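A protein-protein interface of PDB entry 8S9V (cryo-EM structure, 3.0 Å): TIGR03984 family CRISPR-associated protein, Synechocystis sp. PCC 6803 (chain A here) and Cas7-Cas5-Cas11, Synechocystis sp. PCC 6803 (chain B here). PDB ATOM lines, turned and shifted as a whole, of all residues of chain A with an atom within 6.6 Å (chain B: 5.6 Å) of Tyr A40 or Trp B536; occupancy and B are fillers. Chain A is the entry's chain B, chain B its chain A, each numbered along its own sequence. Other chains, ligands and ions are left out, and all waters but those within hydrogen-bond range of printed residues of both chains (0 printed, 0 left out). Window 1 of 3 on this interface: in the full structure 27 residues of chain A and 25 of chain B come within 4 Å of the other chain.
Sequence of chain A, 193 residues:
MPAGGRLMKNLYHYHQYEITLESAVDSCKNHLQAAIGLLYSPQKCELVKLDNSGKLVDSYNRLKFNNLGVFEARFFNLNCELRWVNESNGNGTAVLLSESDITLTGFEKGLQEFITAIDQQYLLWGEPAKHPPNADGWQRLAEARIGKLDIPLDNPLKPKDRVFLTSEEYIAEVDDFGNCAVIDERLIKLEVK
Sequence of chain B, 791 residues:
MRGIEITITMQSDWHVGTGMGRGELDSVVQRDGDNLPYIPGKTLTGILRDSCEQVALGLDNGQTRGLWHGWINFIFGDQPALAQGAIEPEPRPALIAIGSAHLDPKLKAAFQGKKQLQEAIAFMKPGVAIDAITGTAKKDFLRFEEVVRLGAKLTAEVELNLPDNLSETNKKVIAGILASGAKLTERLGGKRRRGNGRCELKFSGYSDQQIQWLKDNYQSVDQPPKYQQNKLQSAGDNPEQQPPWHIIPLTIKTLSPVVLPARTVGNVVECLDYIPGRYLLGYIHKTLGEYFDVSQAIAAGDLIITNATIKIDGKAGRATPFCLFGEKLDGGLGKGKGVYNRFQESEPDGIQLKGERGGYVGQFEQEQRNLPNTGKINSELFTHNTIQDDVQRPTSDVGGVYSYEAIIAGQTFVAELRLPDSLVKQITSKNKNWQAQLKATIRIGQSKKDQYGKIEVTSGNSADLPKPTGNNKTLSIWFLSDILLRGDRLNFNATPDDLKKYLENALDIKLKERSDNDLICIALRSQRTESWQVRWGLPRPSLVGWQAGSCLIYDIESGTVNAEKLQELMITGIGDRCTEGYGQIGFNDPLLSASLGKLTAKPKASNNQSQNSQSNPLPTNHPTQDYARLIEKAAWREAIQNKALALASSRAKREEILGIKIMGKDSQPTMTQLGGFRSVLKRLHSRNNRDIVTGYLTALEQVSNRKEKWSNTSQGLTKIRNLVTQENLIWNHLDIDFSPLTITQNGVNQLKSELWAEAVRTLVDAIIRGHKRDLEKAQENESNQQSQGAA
OE1 of Gln A43 sits at hydrogen-bond distance from NH2 of Arg B535. NE2 of Gln B533 sits at hydrogen-bond distance from O of Pro A42. The backbone carbonyl oxygen of Ser A41 is in hydrogen-bond range of the indole nitrogen of Trp B536 (2.7 Å).
The backbone NH of Tyr A40 lies within hydrogen-bond range of the backbone carbonyl oxygen of Glu A72. The backbone carbonyl oxygen (O) of Leu A68 is in hydrogen-bond range of the side-chain hydroxyl (OG) of Ser A41, 2.8 Å away. The backbone NH (N) of Gln B533 is in hydrogen-bond range of the backbone carbonyl oxygen (O) of Leu B538. The side-chain hydroxyl of Ser A41 lies close to the backbone NH of Gln A43 (3.4 Å). The backbone carbonyl oxygen of Tyr A40 lies within hydrogen-bond range of the backbone NH of Phe A71 (2.8 Å).
Tyr A40 touches Trp B536 (CD1 to CH2, 3.8 Å). Pro A42 touches Arg B535 (O to CD, 3.6 Å). Gln A43 touches Trp B536. CA of Lys A44 touches CD1 of Trp B536, 3.6 Å away. Cys A45 touches Trp B536 (CB to CD2, 3.8 Å).
Of chain B, only Trp B536 comes within 4 Å of Tyr A40. Of the printed residues of chain A, Trp B536 touches Tyr A40, Ser A41, Gln A43, Lys A44 and Cys A45. Printed residues of chain B within 4 Å of Gln A43: Arg B535 and Trp B536. Printed residues of chain B within 4 Å of Lys A44: Trp B536 (3.6 Å). Of the printed residues of chain B, Pro A42 touches Gln B533 and Arg B535. Of the printed residues of chain B, Ser A41 touches Trp B536. Val A70 touches none of the printed residues of chain B. Phe A71 touches none of the printed residues of chain B. The nearest printed residue of chain A that does not touch Trp B536 is Pro A42 (4.01 Å). The nearest printed residue of chain B that does not touch Pro A42 is Trp B536 (4.01 Å).
Along chain A the printed residues that touch a printed residue of chain B span positions 40 to 45. Among the printed residues, no Asp or Glu carboxylate lies within 4 Å of a Lys or Arg side-chain nitrogen of the other chain.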
ATOM      1  N   LEU A  38       3.537 -34.966  21.151  1.00  0.00           N
ATOM      2  CA  LEU A  38       4.224 -33.687  21.153  1.00  0.00           C
ATOM      3  C   LEU A  38       4.611 -33.382  19.717  1.00  0.00           C
ATOM      4  O   LEU A  38       5.518 -34.010  19.174  1.00  0.00           O
ATOM      5  CB  LEU A  38       5.428 -33.723  22.083  1.00  0.00           C
ATOM      6  CG  LEU A  38       6.316 -32.510  22.259  1.00  0.00           C
ATOM      7  CD1 LEU A  38       5.550 -31.338  22.770  1.00  0.00           C
ATOM      8  CD2 LEU A  38       7.354 -32.897  23.265  1.00  0.00           C
ATOM      9  N   LEU A  39       3.916 -32.439  19.103  1.00  0.00           N
ATOM     10  CA  LEU A  39       4.005 -32.180  17.679  1.00  0.00           C
ATOM     11  C   LEU A  39       4.749 -30.877  17.455  1.00  0.00           C
ATOM     12  O   LEU A  39       4.385 -29.851  18.026  1.00  0.00           O
ATOM     13  CB  LEU A  39       2.615 -32.082  17.068  1.00  0.00           C
ATOM     14  CG  LEU A  39       1.612 -33.163  17.428  1.00  0.00           C
ATOM     15  CD1 LEU A  39       0.328 -32.891  16.720  1.00  0.00           C
ATOM     16  CD2 LEU A  39       2.127 -34.501  17.042  1.00  0.00           C
ATOM     17  N   TYR A  40       5.754 -30.904  16.592  1.00  0.00           N
ATOM     18  CA  TYR A  40       6.542 -29.725  16.281  1.00  0.00           C
ATOM     19  C   TYR A  40       6.132 -29.186  14.932  1.00  0.00           C
ATOM     20  O   TYR A  40       6.125 -29.915  13.948  1.00  0.00           O
ATOM     21  CB  TYR A  40       8.031 -30.027  16.253  1.00  0.00           C
ATOM     22  CG  TYR A  40       8.630 -30.552  17.520  1.00  0.00           C
ATOM     23  CD1 TYR A  40       8.059 -30.306  18.737  1.00  0.00           C
ATOM     24  CD2 TYR A  40       9.769 -31.312  17.487  1.00  0.00           C
ATOM     25  CE1 TYR A  40       8.615 -30.790  19.874  1.00  0.00           C
ATOM     26  CE2 TYR A  40      10.317 -31.797  18.620  1.00  0.00           C
ATOM     27  CZ  TYR A  40       9.740 -31.535  19.808  1.00  0.00           C
ATOM     28  OH  TYR A  40      10.311 -32.023  20.944  1.00  0.00           O
ATOM     29  N   SER A  41       5.764 -27.923  14.906  1.00  0.00           N
ATOM     30  CA  SER A  41       5.381 -27.188  13.719  1.00  0.00           C
ATOM     31  C   SER A  41       6.113 -25.860  13.737  1.00  0.00           C
ATOM     32  O   SER A  41       6.556 -25.404  14.793  1.00  0.00           O
ATOM     33  CB  SER A  41       3.866 -26.975  13.683  1.00  0.00           C
ATOM     34  OG  SER A  41       3.539 -25.789  12.993  1.00  0.00           O
ATOM     35  N   PRO A  42       6.295 -25.233  12.580  1.00  0.00           N
ATOM     36  CA  PRO A  42       7.008 -23.952  12.551  1.00  0.00           C
ATOM     37  C   PRO A  42       6.391 -22.866  13.400  1.00  0.00           C
ATOM     38  O   PRO A  42       7.118 -21.990  13.870  1.00  0.00           O
ATOM     39  CB  PRO A  42       6.961 -23.582  11.071  1.00  0.00           C
ATOM     40  CG  PRO A  42       6.910 -24.871  10.401  1.00  0.00           C
ATOM     41  CD  PRO A  42       6.017 -25.715  11.228  1.00  0.00           C
ATOM     42  N   GLN A  43       5.078 -22.869  13.594  1.00  0.00           N
ATOM     43  CA  GLN A  43       4.437 -21.851  14.411  1.00  0.00           C
ATOM     44  C   GLN A  43       4.279 -22.236  15.872  1.00  0.00           C
ATOM     45  O   GLN A  43       4.343 -21.354  16.730  1.00  0.00           O
ATOM     46  CB  GLN A  43       3.063 -21.518  13.831  1.00  0.00           C
ATOM     47  CG  GLN A  43       2.988 -20.274  12.968  1.00  0.00           C
ATOM     48  CD  GLN A  43       3.351 -19.017  13.719  1.00  0.00           C
ATOM     49  OE1 GLN A  43       4.059 -18.156  13.210  1.00  0.00           O
ATOM     50  NE2 GLN A  43       2.881 -18.911  14.947  1.00  0.00           N
ATOM     51  N   LYS A  44       4.031 -23.503  16.193  1.00  0.00           N
ATOM     52  CA  LYS A  44       3.736 -23.865  17.574  1.00  0.00           C
ATOM     53  C   LYS A  44       4.135 -25.303  17.864  1.00  0.00           C
ATOM     54  O   LYS A  44       4.228 -26.134  16.970  1.00  0.00           O
ATOM     55  CB  LYS A  44       2.273 -23.603  17.894  1.00  0.00           C
ATOM     56  CG  LYS A  44       1.304 -24.319  17.017  1.00  0.00           C
ATOM     57  CD  LYS A  44      -0.106 -23.927  17.377  1.00  0.00           C
ATOM     58  CE  LYS A  44      -1.075 -24.506  16.380  1.00  0.00           C
ATOM     59  NZ  LYS A  44      -2.485 -24.125  16.653  1.00  0.00           N
ATOM     60  N   CYS A  45       4.351 -25.582  19.146  1.00  0.00           N
ATOM     61  CA  CYS A  45       4.615 -26.919  19.667  1.00  0.00           C
ATOM     62  C   CYS A  45       3.427 -27.375  20.504  1.00  0.00           C
ATOM     63  O   CYS A  45       3.117 -26.767  21.530  1.00  0.00           O
ATOM     64  CB  CYS A  45       5.889 -26.911  20.504  1.00  0.00           C
ATOM     65  SG  CYS A  45       6.229 -28.375  21.456  1.00  0.00           S
ATOM     66  N   GLU A  46       2.776 -28.445  20.074  1.00  0.00           N
ATOM     67  CA  GLU A  46       1.479 -28.844  20.592  1.00  0.00           C
ATOM     68  C   GLU A  46       1.601 -30.141  21.368  1.00  0.00           C
ATOM     69  O   GLU A  46       2.137 -31.119  20.852  1.00  0.00           O
ATOM     70  CB  GLU A  46       0.487 -29.057  19.458  1.00  0.00           C
ATOM     71  CG  GLU A  46       0.416 -27.946  18.465  1.00  0.00           C
ATOM     72  CD  GLU A  46      -0.517 -28.282  17.336  1.00  0.00           C
ATOM     73  OE1 GLU A  46      -1.688 -28.601  17.626  1.00  0.00           O
ATOM     74  OE2 GLU A  46      -0.073 -28.268  16.168  1.00  0.00           O
ATOM     75  N   LEU A  68       2.442 -25.134   6.937  1.00  0.00           N
ATOM     76  CA  LEU A  68       3.011 -24.920   8.262  1.00  0.00           C
ATOM     77  C   LEU A  68       2.685 -26.069   9.194  1.00  0.00           C
ATOM     78  O   LEU A  68       2.481 -25.872  10.388  1.00  0.00           O
ATOM     79  CB  LEU A  68       2.570 -23.596   8.876  1.00  0.00           C
ATOM     80  CG  LEU A  68       2.793 -22.345   8.048  1.00  0.00           C
ATOM     81  CD1 LEU A  68       2.027 -21.222   8.646  1.00  0.00           C
ATOM     82  CD2 LEU A  68       4.236 -22.004   8.040  1.00  0.00           C
ATOM     83  N   GLY A  69       2.575 -27.264   8.642  1.00  0.00           N
ATOM     84  CA  GLY A  69       2.186 -28.412   9.416  1.00  0.00           C
ATOM     85  C   GLY A  69       3.292 -28.909  10.310  1.00  0.00           C
ATOM     86  O   GLY A  69       4.387 -28.361  10.378  1.00  0.00           O
ATOM     87  N   VAL A  70       2.980 -29.995  11.007  1.00  0.00           N
ATOM     88  CA  VAL A  70       3.926 -30.660  11.887  1.00  0.00           C
ATOM     89  C   VAL A  70       4.989 -31.380  11.076  1.00  0.00           C
ATOM     90  O   VAL A  70       4.685 -32.122  10.138  1.00  0.00           O
ATOM     91  CB  VAL A  70       3.190 -31.633  12.807  1.00  0.00           C
ATOM     92  CG1 VAL A  70       2.231 -32.399  12.008  1.00  0.00           C
ATOM     93  CG2 VAL A  70       4.158 -32.581  13.392  1.00  0.00           C
ATOM     94  N   PHE A  71       6.245 -31.160  11.440  1.00  0.00           N
ATOM     95  CA  PHE A  71       7.385 -31.769  10.789  1.00  0.00           C
ATOM     96  C   PHE A  71       8.080 -32.823  11.629  1.00  0.00           C
ATOM     97  O   PHE A  71       8.874 -33.586  11.085  1.00  0.00           O
ATOM     98  CB  PHE A  71       8.396 -30.701  10.368  1.00  0.00           C
ATOM     99  CG  PHE A  71       8.983 -29.920  11.488  1.00  0.00           C
ATOM    100  CD1 PHE A  71       9.967 -30.442  12.278  1.00  0.00           C
ATOM    101  CD2 PHE A  71       8.611 -28.631  11.698  1.00  0.00           C
ATOM    102  CE1 PHE A  71      10.524 -29.697  13.274  1.00  0.00           C
ATOM    103  CE2 PHE A  71       9.170 -27.900  12.690  1.00  0.00           C
ATOM    104  CZ  PHE A  71      10.119 -28.430  13.477  1.00  0.00           C
ATOM    105  N   GLU A  72       7.830 -32.860  12.931  1.00  0.00           N
ATOM    106  CA  GLU A  72       8.367 -33.861  13.836  1.00  0.00           C
ATOM    107  C   GLU A  72       7.347 -34.135  14.923  1.00  0.00           C
ATOM    108  O   GLU A  72       6.632 -33.233  15.346  1.00  0.00           O
ATOM    109  CB  GLU A  72       9.652 -33.404  14.500  1.00  0.00           C
ATOM    110  CG  GLU A  72      10.054 -34.355  15.583  1.00  0.00           C
ATOM    111  CD  GLU A  72      11.428 -34.112  16.136  1.00  0.00           C
ATOM    112  OE1 GLU A  72      12.028 -33.071  15.811  1.00  0.00           O
ATOM    113  OE2 GLU A  72      11.906 -34.972  16.904  1.00  0.00           O
ATOM    114  N   ALA A  73       7.290 -35.378  15.390  1.00  0.00           N
ATOM    115  CA  ALA A  73       6.347 -35.745  16.435  1.00  0.00           C
ATOM    116  C   ALA A  73       6.956 -36.812  17.327  1.00  0.00           C
ATOM    117  O   ALA A  73       7.808 -37.581  16.895  1.00  0.00           O
ATOM    118  CB  ALA A  73       5.043 -36.259  15.845  1.00  0.00           C
ATOM    119  N   ARG A  74       6.530 -36.835  18.581  1.00  0.00           N
ATOM    120  CA  ARG A  74       6.816 -37.920  19.504  1.00  0.00           C
ATOM    121  C   ARG A  74       5.511 -38.353  20.139  1.00  0.00           C
ATOM    122  O   ARG A  74       4.740 -37.515  20.599  1.00  0.00           O
ATOM    123  CB  ARG A  74       7.784 -37.472  20.584  1.00  0.00           C
ATOM    124  CG  ARG A  74       9.071 -36.914  20.040  1.00  0.00           C
ATOM    125  CD  ARG A  74      10.013 -36.482  21.134  1.00  0.00           C
ATOM    126  NE  ARG A  74      10.602 -37.609  21.841  1.00  0.00           N
ATOM    127  CZ  ARG A  74      11.735 -37.537  22.528  1.00  0.00           C
ATOM    128  NH1 ARG A  74      12.215 -38.604  23.149  1.00  0.00           N
ATOM    129  NH2 ARG A  74      12.397 -36.393  22.581  1.00  0.00           N
ATOM    130  N   GLN B 533      12.914 -20.889  20.791  1.00  0.00           N
ATOM    131  CA  GLN B 533      12.193 -20.528  19.581  1.00  0.00           C
ATOM    132  C   GLN B 533      11.084 -19.550  19.885  1.00  0.00           C
ATOM    133  O   GLN B 533      10.115 -19.897  20.550  1.00  0.00           O
ATOM    134  CB  GLN B 533      11.615 -21.723  18.853  1.00  0.00           C
ATOM    135  CG  GLN B 533      10.651 -21.214  17.839  1.00  0.00           C
ATOM    136  CD  GLN B 533      10.584 -22.036  16.627  1.00  0.00           C
ATOM    137  OE1 GLN B 533      11.258 -23.035  16.526  1.00  0.00           O
ATOM    138  NE2 GLN B 533       9.741 -21.653  15.699  1.00  0.00           N
ATOM    139  N   VAL B 534      11.204 -18.356  19.325  1.00  0.00           N
ATOM    140  CA  VAL B 534      10.316 -17.255  19.640  1.00  0.00           C
ATOM    141  C   VAL B 534       8.894 -17.517  19.187  1.00  0.00           C
ATOM    142  O   VAL B 534       7.942 -17.089  19.838  1.00  0.00           O
ATOM    143  CB  VAL B 534      10.869 -15.980  19.011  1.00  0.00           C
ATOM    144  CG1 VAL B 534       9.988 -14.854  19.360  1.00  0.00           C
ATOM    145  CG2 VAL B 534      12.260 -15.743  19.513  1.00  0.00           C
ATOM    146  N   ARG B 535       8.711 -18.173  18.052  1.00  0.00           N
ATOM    147  CA  ARG B 535       7.354 -18.459  17.605  1.00  0.00           C
ATOM    148  C   ARG B 535       6.641 -19.416  18.547  1.00  0.00           C
ATOM    149  O   ARG B 535       5.455 -19.240  18.824  1.00  0.00           O
ATOM    150  CB  ARG B 535       7.383 -18.999  16.192  1.00  0.00           C
ATOM    151  CG  ARG B 535       7.888 -17.990  15.219  1.00  0.00           C
ATOM    152  CD  ARG B 535       7.786 -18.475  13.819  1.00  0.00           C
ATOM    153  NE  ARG B 535       8.292 -17.482  12.895  1.00  0.00           N
ATOM    154  CZ  ARG B 535       7.653 -16.372  12.578  1.00  0.00           C
ATOM    155  NH1 ARG B 535       8.234 -15.463  11.821  1.00  0.00           N
ATOM    156  NH2 ARG B 535       6.465 -16.140  13.093  1.00  0.00           N
ATOM    157  N   TRP B 536       7.336 -20.442  19.034  1.00  0.00           N
ATOM    158  CA  TRP B 536       6.736 -21.392  19.958  1.00  0.00           C
ATOM    159  C   TRP B 536       6.515 -20.789  21.322  1.00  0.00           C
ATOM    160  O   TRP B 536       5.552 -21.137  22.003  1.00  0.00           O
ATOM    161  CB  TRP B 536       7.631 -22.598  20.152  1.00  0.00           C
ATOM    162  CG  TRP B 536       7.808 -23.483  19.033  1.00  0.00           C
ATOM    163  CD1 TRP B 536       7.291 -23.360  17.811  1.00  0.00           C
ATOM    164  CD2 TRP B 536       8.586 -24.668  19.032  1.00  0.00           C
ATOM    165  NE1 TRP B 536       7.685 -24.405  17.023  1.00  0.00           N
ATOM    166  CE2 TRP B 536       8.490 -25.225  17.760  1.00  0.00           C
ATOM    167  CE3 TRP B 536       9.361 -25.309  19.989  1.00  0.00           C
ATOM    168  CZ2 TRP B 536       9.134 -26.384  17.416  1.00  0.00           C
ATOM    169  CZ3 TRP B 536       9.991 -26.447  19.652  1.00  0.00           C
ATOM    170  CH2 TRP B 536       9.881 -26.983  18.378  1.00  0.00           C
ATOM    171  N   GLY B 537       7.396 -19.899  21.739  1.00  0.00           N
ATOM    172  CA  GLY B 537       7.433 -19.475  23.116  1.00  0.00           C
ATOM    173  C   GLY B 537       7.958 -20.507  24.071  1.00  0.00           C
ATOM    174  O   GLY B 537       7.661 -20.432  25.256  1.00  0.00           O
ATOM    175  N   LEU B 538       8.755 -21.458  23.590  1.00  0.00           N
ATOM    176  CA  LEU B 538       9.359 -22.531  24.364  1.00  0.00           C
ATOM    177  C   LEU B 538      10.734 -22.779  23.775  1.00  0.00           C
ATOM    178  O   LEU B 538      10.922 -22.592  22.573  1.00  0.00           O
ATOM    179  CB  LEU B 538       8.523 -23.803  24.277  1.00  0.00           C
ATOM    180  CG  LEU B 538       7.164 -23.721  24.919  1.00  0.00           C
ATOM    181  CD1 LEU B 538       6.462 -24.996  24.679  1.00  0.00           C
ATOM    182  CD2 LEU B 538       7.341 -23.492  26.363  1.00  0.00           C
ATOM    183  N   PRO B 539      11.677 -23.291  24.550  1.00  0.00           N
ATOM    184  CA  PRO B 539      12.979 -23.604  23.976  1.00  0.00           C
ATOM    185  C   PRO B 539      12.885 -24.658  22.896  1.00  0.00           C
ATOM    186  O   PRO B 539      12.007 -25.510  22.914  1.00  0.00           O
ATOM    187  CB  PRO B 539      13.785 -24.079  25.184  1.00  0.00           C
ATOM    188  CG  PRO B 539      12.815 -24.541  26.111  1.00  0.00           C
ATOM    189  CD  PRO B 539      11.620 -23.685  25.959  1.00  0.00           C
ATOM    190  N   ARG B 540      13.804 -24.589  21.942  1.00  0.00           N
ATOM    191  CA  ARG B 540      13.931 -25.645  20.963  1.00  0.00           C
ATOM    192  C   ARG B 540      14.313 -26.948  21.647  1.00  0.00           C
ATOM    193  O   ARG B 540      14.915 -26.943  22.719  1.00  0.00           O
ATOM    194  CB  ARG B 540      14.981 -25.275  19.929  1.00  0.00           C
ATOM    195  CG  ARG B 540      14.616 -24.136  19.053  1.00  0.00           C
ATOM    196  CD  ARG B 540      15.826 -23.687  18.275  1.00  0.00           C
ATOM    197  NE  ARG B 540      16.172 -24.437  17.097  1.00  0.00           N
ATOM    198  CZ  ARG B 540      17.180 -24.105  16.307  1.00  0.00           C
ATOM    199  NH1 ARG B 540      17.352 -24.684  15.141  1.00  0.00           N
ATOM    200  NH2 ARG B 540      17.975 -23.125  16.662  1.00  0.00           N
ATOM    201  N   PRO B 541      13.985 -28.077  21.038  1.00  0.00           N
ATOM    202  CA  PRO B 541      14.647 -29.319  21.407  1.00  0.00           C
ATOM    203  C   PRO B 541      16.150 -29.177  21.289  1.00  0.00           C
ATOM    204  O   PRO B 541      16.658 -28.526  20.382  1.00  0.00           O
ATOM    205  CB  PRO B 541      14.088 -30.317  20.402  1.00  0.00           C
ATOM    206  CG  PRO B 541      13.724 -29.511  19.272  1.00  0.00           C
ATOM    207  CD  PRO B 541      13.179 -28.253  19.830  1.00  0.00           C
